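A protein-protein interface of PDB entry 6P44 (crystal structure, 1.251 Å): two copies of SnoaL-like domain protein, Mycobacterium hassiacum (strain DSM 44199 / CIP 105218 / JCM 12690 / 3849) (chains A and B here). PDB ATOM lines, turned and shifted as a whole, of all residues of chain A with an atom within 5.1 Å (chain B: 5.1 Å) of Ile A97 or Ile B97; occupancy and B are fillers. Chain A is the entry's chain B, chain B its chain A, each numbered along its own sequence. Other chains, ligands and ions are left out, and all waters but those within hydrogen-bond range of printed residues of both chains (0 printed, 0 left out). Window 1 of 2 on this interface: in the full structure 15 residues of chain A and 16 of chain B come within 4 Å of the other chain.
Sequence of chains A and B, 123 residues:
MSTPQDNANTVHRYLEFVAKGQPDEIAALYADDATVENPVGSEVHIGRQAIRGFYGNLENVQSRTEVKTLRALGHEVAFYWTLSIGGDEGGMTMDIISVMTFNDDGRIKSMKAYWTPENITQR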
ATOM      1  N   THR A  69     -15.679   6.623  19.261  1.00  0.00           N
ATOM      2  CA  THR A  69     -15.706   5.272  19.783  1.00  0.00           C
ATOM      3  C   THR A  69     -14.297   4.712  19.686  1.00  0.00           C
ATOM      4  O   THR A  69     -13.534   5.042  18.769  1.00  0.00           O
ATOM      5  CB  THR A  69     -16.726   4.388  19.040  1.00  0.00           C
ATOM      6  OG1 THR A  69     -16.750   3.079  19.623  1.00  0.00           O
ATOM      7  CG2 THR A  69     -16.408   4.275  17.568  1.00  0.00           C
ATOM      8  N   ARG A  71     -12.059   0.947  20.498  1.00  0.00           N
ATOM      9  CA  ARG A  71     -12.104  -0.484  20.784  1.00  0.00           C
ATOM     10  C   ARG A  71     -10.676  -0.992  20.932  1.00  0.00           C
ATOM     11  O   ARG A  71      -9.949  -1.133  19.934  1.00  0.00           O
ATOM     12  CB  ARG A  71     -12.847  -1.266  19.690  1.00  0.00           C
ATOM     13  CG  ARG A  71     -14.332  -0.902  19.543  1.00  0.00           C
ATOM     14  CD  ARG A  71     -14.592  -0.036  18.350  1.00  0.00           C
ATOM     15  NE  ARG A  71     -15.896   0.637  18.367  1.00  0.00           N
ATOM     16  CZ  ARG A  71     -17.019   0.200  17.791  1.00  0.00           C
ATOM     17  NH1 ARG A  71     -17.060  -0.941  17.135  1.00  0.00           N
ATOM     18  NH2 ARG A  71     -18.129   0.926  17.884  1.00  0.00           N
ATOM     19  N   ALA A  78      -8.577   0.319  17.673  1.00  0.00           N
ATOM     20  CA  ALA A  78      -9.227   1.019  16.571  1.00  0.00           C
ATOM     21  C   ALA A  78     -10.068   2.120  17.171  1.00  0.00           C
ATOM     22  O   ALA A  78     -10.794   1.885  18.143  1.00  0.00           O
ATOM     23  CB  ALA A  78     -10.121   0.095  15.750  1.00  0.00           C
ATOM     24  N   PHE A  79      -9.961   3.325  16.620  1.00  0.00           N
ATOM     25  CA  PHE A  79     -10.693   4.454  17.176  1.00  0.00           C
ATOM     26  C   PHE A  79     -11.169   5.384  16.080  1.00  0.00           C
ATOM     27  O   PHE A  79     -10.471   5.611  15.090  1.00  0.00           O
ATOM     28  CB  PHE A  79      -9.932   5.203  18.285  1.00  0.00           C
ATOM     29  CG  PHE A  79      -8.518   5.633  17.950  1.00  0.00           C
ATOM     30  CD1 PHE A  79      -7.475   4.720  17.825  1.00  0.00           C
ATOM     31  CD2 PHE A  79      -8.224   6.978  17.828  1.00  0.00           C
ATOM     32  CE1 PHE A  79      -6.167   5.156  17.573  1.00  0.00           C
ATOM     33  CE2 PHE A  79      -6.924   7.404  17.556  1.00  0.00           C
ATOM     34  CZ  PHE A  79      -5.910   6.495  17.448  1.00  0.00           C
ATOM     35  N   TYR A  80     -12.388   5.877  16.258  1.00  0.00           N
ATOM     36  CA  TYR A  80     -13.023   6.815  15.345  1.00  0.00           C
ATOM     37  C   TYR A  80     -13.134   8.127  16.111  1.00  0.00           C
ATOM     38  O   TYR A  80     -13.658   8.150  17.232  1.00  0.00           O
ATOM     39  CB  TYR A  80     -14.398   6.260  14.963  1.00  0.00           C
ATOM     40  CG  TYR A  80     -15.203   7.044  13.955  1.00  0.00           C
ATOM     41  CD1 TYR A  80     -14.604   7.778  12.940  1.00  0.00           C
ATOM     42  CD2 TYR A  80     -16.588   7.048  14.026  1.00  0.00           C
ATOM     43  CE1 TYR A  80     -15.372   8.484  12.024  1.00  0.00           C
ATOM     44  CE2 TYR A  80     -17.349   7.752  13.118  1.00  0.00           C
ATOM     45  CZ  TYR A  80     -16.741   8.467  12.121  1.00  0.00           C
ATOM     46  OH  TYR A  80     -17.512   9.178  11.212  1.00  0.00           O
ATOM     47  N   TRP A  81     -12.555   9.190  15.556  1.00  0.00           N
ATOM     48  CA  TRP A  81     -12.313  10.399  16.325  1.00  0.00           C
ATOM     49  C   TRP A  81     -12.316  11.614  15.414  1.00  0.00           C
ATOM     50  O   TRP A  81     -12.262  11.501  14.189  1.00  0.00           O
ATOM     51  CB  TRP A  81     -11.004  10.300  17.101  1.00  0.00           C
ATOM     52  CG  TRP A  81      -9.773  10.148  16.258  1.00  0.00           C
ATOM     53  CD1 TRP A  81      -9.398   9.053  15.535  1.00  0.00           C
ATOM     54  CD2 TRP A  81      -8.733  11.115  16.086  1.00  0.00           C
ATOM     55  NE1 TRP A  81      -8.191   9.276  14.928  1.00  0.00           N
ATOM     56  CE2 TRP A  81      -7.753  10.533  15.255  1.00  0.00           C
ATOM     57  CE3 TRP A  81      -8.523  12.411  16.569  1.00  0.00           C
ATOM     58  CZ2 TRP A  81      -6.590  11.209  14.883  1.00  0.00           C
ATOM     59  CZ3 TRP A  81      -7.376  13.083  16.198  1.00  0.00           C
ATOM     60  CH2 TRP A  81      -6.420  12.483  15.374  1.00  0.00           C
ATOM     61  N   ASP A  95     -12.554  13.927  10.271  1.00  0.00           N
ATOM     62  CA  ASP A  95     -13.281  12.771  10.783  1.00  0.00           C
ATOM     63  C   ASP A  95     -12.482  11.532  10.390  1.00  0.00           C
ATOM     64  O   ASP A  95     -12.441  11.169   9.211  1.00  0.00           O
ATOM     65  CB  ASP A  95     -14.677  12.771  10.166  1.00  0.00           C
ATOM     66  CG  ASP A  95     -15.593  11.748  10.786  1.00  0.00           C
ATOM     67  OD1 ASP A  95     -15.656  11.691  12.024  1.00  0.00           O
ATOM     68  OD2 ASP A  95     -16.277  11.020  10.034  1.00  0.00           O
ATOM     69  N   ILE A  96     -11.787  10.866  11.569  1.00  0.00           N
ATOM     70  CA  ILE A  96     -10.732   9.951  11.139  1.00  0.00           C
ATOM     71  C   ILE A  96     -10.952   8.591  11.784  1.00  0.00           C
ATOM     72  O   ILE A  96     -11.239   8.506  12.982  1.00  0.00           O
ATOM     73  CB  ILE A  96      -9.349  10.487  11.575  1.00  0.00           C
ATOM     74  CG1 ILE A  96      -9.103  11.895  11.021  1.00  0.00           C
ATOM     75  CG2 ILE A  96      -8.224   9.521  11.161  1.00  0.00           C
ATOM     76  CD1 ILE A  96      -7.944  12.615  11.695  1.00  0.00           C
ATOM     77  N   ILE A  97     -10.740   7.521  11.012  1.00  0.00           N
ATOM     78  CA  ILE A  97     -10.651   6.165  11.563  1.00  0.00           C
ATOM     79  C   ILE A  97      -9.174   5.821  11.657  1.00  0.00           C
ATOM     80  O   ILE A  97      -8.456   5.888  10.652  1.00  0.00           O
ATOM     81  CB  ILE A  97     -11.391   5.117  10.710  1.00  0.00           C
ATOM     82  CG1 ILE A  97     -12.888   5.404  10.652  1.00  0.00           C
ATOM     83  CG2 ILE A  97     -11.143   3.706  11.267  1.00  0.00           C
ATOM     84  CD1 ILE A  97     -13.642   4.536   9.669  1.00  0.00           C
ATOM     85  N   SER A  98      -8.724   5.439  12.852  1.00  0.00           N
ATOM     86  CA  SER A  98      -7.331   5.110  13.087  1.00  0.00           C
ATOM     87  C   SER A  98      -7.212   3.727  13.705  1.00  0.00           C
ATOM     88  O   SER A  98      -8.071   3.283  14.461  1.00  0.00           O
ATOM     89  CB  SER A  98      -6.683   6.084  14.042  1.00  0.00           C
ATOM     90  OG  SER A  98      -6.626   7.373  13.458  1.00  0.00           O
ATOM     91  N   VAL A  99      -6.113   3.042  13.384  1.00  0.00           N
ATOM     92  CA  VAL A  99      -5.739   1.795  14.050  1.00  0.00           C
ATOM     93  C   VAL A  99      -4.289   1.901  14.489  1.00  0.00           C
ATOM     94  O   VAL A  99      -3.404   2.221  13.684  1.00  0.00           O
ATOM     95  CB  VAL A  99      -5.916   0.573  13.125  1.00  0.00           C
ATOM     96  CG1 VAL A  99      -5.425  -0.696  13.800  1.00  0.00           C
ATOM     97  CG2 VAL A  99      -7.374   0.411  12.731  1.00  0.00           C
ATOM     98  N   LYS A 112      -2.007   3.588  11.526  1.00  0.00           N
ATOM     99  CA  LYS A 112      -2.608   3.782  10.214  1.00  0.00           C
ATOM    100  C   LYS A 112      -3.808   4.702  10.397  1.00  0.00           C
ATOM    101  O   LYS A 112      -4.599   4.510  11.323  1.00  0.00           O
ATOM    102  CB  LYS A 112      -3.044   2.450   9.595  1.00  0.00           C
ATOM    103  CG  LYS A 112      -1.896   1.628   9.072  1.00  0.00           C
ATOM    104  CD  LYS A 112      -2.366   0.354   8.390  1.00  0.00           C
ATOM    105  CE  LYS A 112      -1.186  -0.337   7.753  1.00  0.00           C
ATOM    106  NZ  LYS A 112      -1.577  -1.601   7.077  1.00  0.00           N
ATOM    107  N   ALA A 113      -3.935   5.698   9.527  1.00  0.00           N
ATOM    108  CA  ALA A 113      -5.035   6.659   9.576  1.00  0.00           C
ATOM    109  C   ALA A 113      -5.794   6.655   8.253  1.00  0.00           C
ATOM    110  O   ALA A 113      -5.195   6.765   7.178  1.00  0.00           O
ATOM    111  CB  ALA A 113      -4.521   8.071   9.906  1.00  0.00           C
ATOM    112  N   TYR A 114      -7.113   6.523   8.343  1.00  0.00           N
ATOM    113  CA  TYR A 114      -7.983   6.399   7.176  1.00  0.00           C
ATOM    114  C   TYR A 114      -8.903   7.614   7.110  1.00  0.00           C
ATOM    115  O   TYR A 114      -9.861   7.715   7.887  1.00  0.00           O
ATOM    116  CB  TYR A 114      -8.807   5.114   7.251  1.00  0.00           C
ATOM    117  CG  TYR A 114      -8.028   3.812   7.378  1.00  0.00           C
ATOM    118  CD1 TYR A 114      -7.538   3.401   8.604  1.00  0.00           C
ATOM    119  CD2 TYR A 114      -7.806   3.002   6.288  1.00  0.00           C
ATOM    120  CE1 TYR A 114      -6.842   2.224   8.744  1.00  0.00           C
ATOM    121  CE2 TYR A 114      -7.126   1.794   6.416  1.00  0.00           C
ATOM    122  CZ  TYR A 114      -6.633   1.424   7.648  1.00  0.00           C
ATOM    123  OH  TYR A 114      -5.919   0.278   7.835  1.00  0.00           O
ATOM    124  N   THR B  69     -19.624   5.081   7.215  1.00  0.00           N
ATOM    125  CA  THR B  69     -18.559   5.745   6.478  1.00  0.00           C
ATOM    126  C   THR B  69     -17.589   4.679   5.991  1.00  0.00           C
ATOM    127  O   THR B  69     -17.351   3.684   6.676  1.00  0.00           O
ATOM    128  CB  THR B  69     -17.862   6.823   7.327  1.00  0.00           C
ATOM    129  OG1 THR B  69     -16.864   7.508   6.552  1.00  0.00           O
ATOM    130  CG2 THR B  69     -17.211   6.243   8.551  1.00  0.00           C
ATOM    131  N   ARG B  71     -13.802   4.293   3.744  1.00  0.00           N
ATOM    132  CA  ARG B  71     -12.614   4.948   3.196  1.00  0.00           C
ATOM    133  C   ARG B  71     -11.754   3.899   2.501  1.00  0.00           C
ATOM    134  O   ARG B  71     -11.105   3.077   3.164  1.00  0.00           O
ATOM    135  CB  ARG B  71     -11.811   5.663   4.286  1.00  0.00           C
ATOM    136  CG  ARG B  71     -12.552   6.830   4.982  1.00  0.00           C
ATOM    137  CD  ARG B  71     -12.955   6.493   6.380  1.00  0.00           C
ATOM    138  NE  ARG B  71     -13.987   7.383   6.925  1.00  0.00           N
ATOM    139  CZ  ARG B  71     -13.770   8.432   7.709  1.00  0.00           C
ATOM    140  NH1 ARG B  71     -12.554   8.769   8.076  1.00  0.00           N
ATOM    141  NH2 ARG B  71     -14.792   9.146   8.139  1.00  0.00           N
ATOM    142  N   ALA B  78     -11.253   0.848   5.137  1.00  0.00           N
ATOM    143  CA  ALA B  78     -11.737   0.933   6.511  1.00  0.00           C
ATOM    144  C   ALA B  78     -13.190   1.368   6.445  1.00  0.00           C
ATOM    145  O   ALA B  78     -13.533   2.292   5.698  1.00  0.00           O
ATOM    146  CB  ALA B  78     -10.928   1.938   7.337  1.00  0.00           C
ATOM    147  N   PHE B  79     -14.043   0.707   7.215  1.00  0.00           N
ATOM    148  CA  PHE B  79     -15.460   1.029   7.154  1.00  0.00           C
ATOM    149  C   PHE B  79     -16.091   0.874   8.527  1.00  0.00           C
ATOM    150  O   PHE B  79     -15.759  -0.041   9.277  1.00  0.00           O
ATOM    151  CB  PHE B  79     -16.218   0.274   6.038  1.00  0.00           C
ATOM    152  CG  PHE B  79     -16.050  -1.237   6.023  1.00  0.00           C
ATOM    153  CD1 PHE B  79     -14.863  -1.835   5.608  1.00  0.00           C
ATOM    154  CD2 PHE B  79     -17.116  -2.058   6.359  1.00  0.00           C
ATOM    155  CE1 PHE B  79     -14.740  -3.216   5.551  1.00  0.00           C
ATOM    156  CE2 PHE B  79     -17.001  -3.442   6.302  1.00  0.00           C
ATOM    157  CZ  PHE B  79     -15.811  -4.017   5.896  1.00  0.00           C
ATOM    158  N   TYR B  80     -16.980   1.807   8.846  1.00  0.00           N
ATOM    159  CA  TYR B  80     -17.735   1.830  10.089  1.00  0.00           C
ATOM    160  C   TYR B  80     -19.178   1.590   9.683  1.00  0.00           C
ATOM    161  O   TYR B  80     -19.691   2.276   8.789  1.00  0.00           O
ATOM    162  CB  TYR B  80     -17.544   3.192  10.774  1.00  0.00           C
ATOM    163  CG  TYR B  80     -18.254   3.382  12.101  1.00  0.00           C
ATOM    164  CD1 TYR B  80     -18.252   2.394  13.074  1.00  0.00           C
ATOM    165  CD2 TYR B  80     -18.912   4.573  12.385  1.00  0.00           C
ATOM    166  CE1 TYR B  80     -18.892   2.580  14.282  1.00  0.00           C
ATOM    167  CE2 TYR B  80     -19.561   4.768  13.588  1.00  0.00           C
ATOM    168  CZ  TYR B  80     -19.544   3.771  14.538  1.00  0.00           C
ATOM    169  OH  TYR B  80     -20.202   3.953  15.741  1.00  0.00           O
ATOM    170  N   TRP B  81     -19.803   0.577  10.282  1.00  0.00           N
ATOM    171  CA  TRP B  81     -21.055   0.076   9.751  1.00  0.00           C
ATOM    172  C   TRP B  81     -21.868  -0.579  10.853  1.00  0.00           C
ATOM    173  O   TRP B  81     -21.379  -0.848  11.951  1.00  0.00           O
ATOM    174  CB  TRP B  81     -20.815  -0.924   8.614  1.00  0.00           C
ATOM    175  CG  TRP B  81     -20.016  -2.148   8.981  1.00  0.00           C
ATOM    176  CD1 TRP B  81     -18.678  -2.205   9.270  1.00  0.00           C
ATOM    177  CD2 TRP B  81     -20.494  -3.500   9.044  1.00  0.00           C
ATOM    178  NE1 TRP B  81     -18.301  -3.506   9.526  1.00  0.00           N
ATOM    179  CE2 TRP B  81     -19.395  -4.316   9.401  1.00  0.00           C
ATOM    180  CE3 TRP B  81     -21.742  -4.097   8.860  1.00  0.00           C
ATOM    181  CZ2 TRP B  81     -19.502  -5.695   9.527  1.00  0.00           C
ATOM    182  CZ3 TRP B  81     -21.846  -5.461   9.019  1.00  0.00           C
ATOM    183  CH2 TRP B  81     -20.739  -6.244   9.348  1.00  0.00           C
ATOM    184  N   ASP B  95     -22.529  -1.584  16.034  1.00  0.00           N
ATOM    185  CA  ASP B  95     -21.701  -0.701  15.225  1.00  0.00           C
ATOM    186  C   ASP B  95     -20.264  -1.212  15.281  1.00  0.00           C
ATOM    187  O   ASP B  95     -19.687  -1.365  16.365  1.00  0.00           O
ATOM    188  CB  ASP B  95     -21.830   0.781  15.613  1.00  0.00           C
ATOM    189  CG  ASP B  95     -21.518   1.054  17.062  1.00  0.00           C
ATOM    190  OD1 ASP B  95     -22.071   0.375  17.967  1.00  0.00           O
ATOM    191  OD2 ASP B  95     -20.738   1.997  17.292  1.00  0.00           O
ATOM    192  N   ILE B  96     -19.746  -1.512  14.185  1.00  0.00           N
ATOM    193  CA  ILE B  96     -18.491  -2.223  13.984  1.00  0.00           C
ATOM    194  C   ILE B  96     -17.536  -1.333  13.200  1.00  0.00           C
ATOM    195  O   ILE B  96     -17.942  -0.669  12.242  1.00  0.00           O
ATOM    196  CB  ILE B  96     -18.757  -3.532  13.202  1.00  0.00           C
ATOM    197  CG1 ILE B  96     -19.722  -4.441  13.982  1.00  0.00           C
ATOM    198  CG2 ILE B  96     -17.450  -4.259  12.876  1.00  0.00           C
ATOM    199  CD1 ILE B  96     -20.277  -5.602  13.177  1.00  0.00           C
ATOM    200  N   ILE B  97     -16.259  -1.336  13.582  1.00  0.00           N
ATOM    201  CA  ILE B  97     -15.187  -0.803  12.741  1.00  0.00           C
ATOM    202  C   ILE B  97     -14.467  -1.979  12.110  1.00  0.00           C
ATOM    203  O   ILE B  97     -13.997  -2.872  12.829  1.00  0.00           O
ATOM    204  CB  ILE B  97     -14.184   0.049  13.531  1.00  0.00           C
ATOM    205  CG1 ILE B  97     -14.854   1.272  14.145  1.00  0.00           C
ATOM    206  CG2 ILE B  97     -13.031   0.468  12.616  1.00  0.00           C
ATOM    207  CD1 ILE B  97     -13.951   2.058  15.120  1.00  0.00           C
ATOM    208  N   SER B  98     -14.369  -1.983  10.780  1.00  0.00           N
ATOM    209  CA  SER B  98     -13.722  -3.069  10.065  1.00  0.00           C
ATOM    210  C   SER B  98     -12.637  -2.525   9.144  1.00  0.00           C
ATOM    211  O   SER B  98     -12.731  -1.404   8.624  1.00  0.00           O
ATOM    212  CB  SER B  98     -14.707  -3.850   9.214  1.00  0.00           C
ATOM    213  OG  SER B  98     -15.674  -4.495  10.009  1.00  0.00           O
ATOM    214  N   VAL B  99     -11.595  -3.339   8.938  1.00  0.00           N
ATOM    215  CA  VAL B  99     -10.558  -3.048   7.956  1.00  0.00           C
ATOM    216  C   VAL B  99     -10.353  -4.296   7.113  1.00  0.00           C
ATOM    217  O   VAL B  99     -10.121  -5.390   7.652  1.00  0.00           O
ATOM    218  CB  VAL B  99      -9.224  -2.616   8.595  1.00  0.00           C
ATOM    219  CG1 VAL B  99      -8.155  -2.450   7.496  1.00  0.00           C
ATOM    220  CG2 VAL B  99      -9.406  -1.343   9.379  1.00  0.00           C
ATOM    221  N   LYS B 112     -10.261  -7.634   9.521  1.00  0.00           N
ATOM    222  CA  LYS B 112     -10.214  -7.447  10.967  1.00  0.00           C
ATOM    223  C   LYS B 112     -11.450  -6.661  11.369  1.00  0.00           C
ATOM    224  O   LYS B 112     -11.782  -5.658  10.720  1.00  0.00           O
ATOM    225  CB  LYS B 112      -8.966  -6.675  11.397  1.00  0.00           C
ATOM    226  CG  LYS B 112      -7.694  -7.491  11.320  1.00  0.00           C
ATOM    227  CD  LYS B 112      -6.481  -6.775  11.890  1.00  0.00           C
ATOM    228  CE  LYS B 112      -5.281  -7.708  11.906  1.00  0.00           C
ATOM    229  NZ  LYS B 112      -4.025  -7.079  12.336  1.00  0.00           N
ATOM    230  N   ALA B 113     -12.140  -7.130  12.407  1.00  0.00           N
ATOM    231  CA  ALA B 113     -13.366  -6.505  12.890  1.00  0.00           C
ATOM    232  C   ALA B 113     -13.179  -6.119  14.356  1.00  0.00           C
ATOM    233  O   ALA B 113     -12.798  -6.955  15.187  1.00  0.00           O
ATOM    234  CB  ALA B 113     -14.568  -7.439  12.721  1.00  0.00           C
ATOM    235  N   TYR B 114     -13.454  -4.854  14.670  1.00  0.00           N
ATOM    236  CA  TYR B 114     -13.226  -4.292  15.996  1.00  0.00           C
ATOM    237  C   TYR B 114     -14.581  -3.936  16.595  1.00  0.00           C
ATOM    238  O   TYR B 114     -15.192  -2.931  16.218  1.00  0.00           O
ATOM    239  CB  TYR B 114     -12.337  -3.052  15.921  1.00  0.00           C
ATOM    240  CG  TYR B 114     -10.972  -3.238  15.273  1.00  0.00           C
ATOM    241  CD1 TYR B 114     -10.833  -3.240  13.895  1.00  0.00           C
ATOM    242  CD2 TYR B 114      -9.816  -3.351  16.043  1.00  0.00           C
ATOM    243  CE1 TYR B 114      -9.621  -3.380  13.307  1.00  0.00           C
ATOM    244  CE2 TYR B 114      -8.572  -3.497  15.453  1.00  0.00           C
ATOM    245  CZ  TYR B 114      -8.482  -3.519  14.077  1.00  0.00           C
ATOM    246  OH  TYR B 114      -7.278  -3.662  13.436  1.00  0.00           O
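The side-chain carboxylate (OD2) of Asp A95 lies within salt-bridge range of the guanidinium group (NH2) of Arg B71, at 3.1 Å.
The guanidinium group of Arg B71 lies within hydrogen-bond range of the backbone carbonyl oxygen of Tyr A114, 2.9 Å away.
The side-chain carboxylate of Asp B95 lies within salt-bridge range of the guanidinium group of Arg A71 (2.9 Å).
NH1 of Arg A71 lies within hydrogen-bond range of O of Tyr B114 (2.9 Å).
The guanidinium group of Arg B71 sits at hydrogen-bond distance from the side-chain hydroxyl of Thr B69 (2.9 Å).
N of Arg B71 lies within hydrogen-bond range of O of Ala B78.
OD2 of Asp B95 lies within hydrogen-bond range of OH of Tyr B80 (2.6 Å).
The backbone carbonyl oxygen of Ile B97 is in hydrogen-bond range of the backbone NH of Tyr B114 (2.8 Å).
The backbone NH (N) of Lys B112 is in hydrogen-bond range of the backbone carbonyl oxygen (O) of Val B99, at 2.9 Å.
The backbone carbonyl oxygen (O) of Trp A81 is in hydrogen-bond range of the backbone NH (N) of Ile A96 (2.7 Å).
Arg A71 touches Ile B96.
NH1 of Arg A71 touches N of Ile B97, 3.7 Å away.
Tyr B114 touches Ala A78 (CD2 to CB, 3.5 Å).
Tyr B80 touches Tyr A80.
CA of Ile A96 touches NH1 of Arg B71 (3.8 Å).
N of Ile A97 touches NH1 of Arg B71, 3.7 Å away.
CG2 of Ile A97 touches CG2 of Ile B97, at 3.98 Å.
Tyr B114 touches Val A99.
CB of Ala B78 touches CG of Tyr A114, 3.5 Å away.
OH of Tyr A114 touches CG1 of Val B99, at 3.5 Å.
Of the printed residues of chain B, Ile A97 touches Arg B71 (3.7 Å) and Ile B97 (3.98 Å).
Of the printed residues of chain A, Ile B97 touches Arg A71 and Ile A97.
Printed residues of chain B within 4 Å of Val A99: Tyr B114 (3.5 Å).
Of the printed residues of chain B, Asp A95 touches Arg B71.
Printed residues of chain B within 4 Å of Ile A96: Arg B71 (3.8 Å).
Phe B79 touches none of the printed residues of chain A.
Trp B81 touches none of the printed residues of chain A.
The nearest printed residue of chain B that does not touch Ile A97 is Thr B69 (4.1 Å).
The nearest printed residue of chain A that does not touch Val B99 is Val A99 (4.3 Å).
Of the 14 printed residues of chain B, 9 touch a printed residue of chain A.
Hydrophobic or aromatic side chains of chain B that line the printed part of chain A: Ala B78, Tyr B80, Ile B97, Val B99 and Tyr B114.
Hydrophobic or aromatic side chains of chain A that line the printed part of chain B: Ala A78, Tyr A80, Ile A97, Val A99 and Tyr A114.
Among the printed residues, 16 pairs touch across the chains.
Arg A71 touches Ile B97, and with the chains exchanged Ile A97 touches Arg B71.
Arg A71 touches Tyr B114, and with the chains exchanged Tyr A114 touches Arg B71.
Tyr A80 touches Arg B71, but with the chains exchanged Arg A71 does not touch Tyr B80 (4.04 Å).
Tyr A80 touches its own counterpart, Tyr B80.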
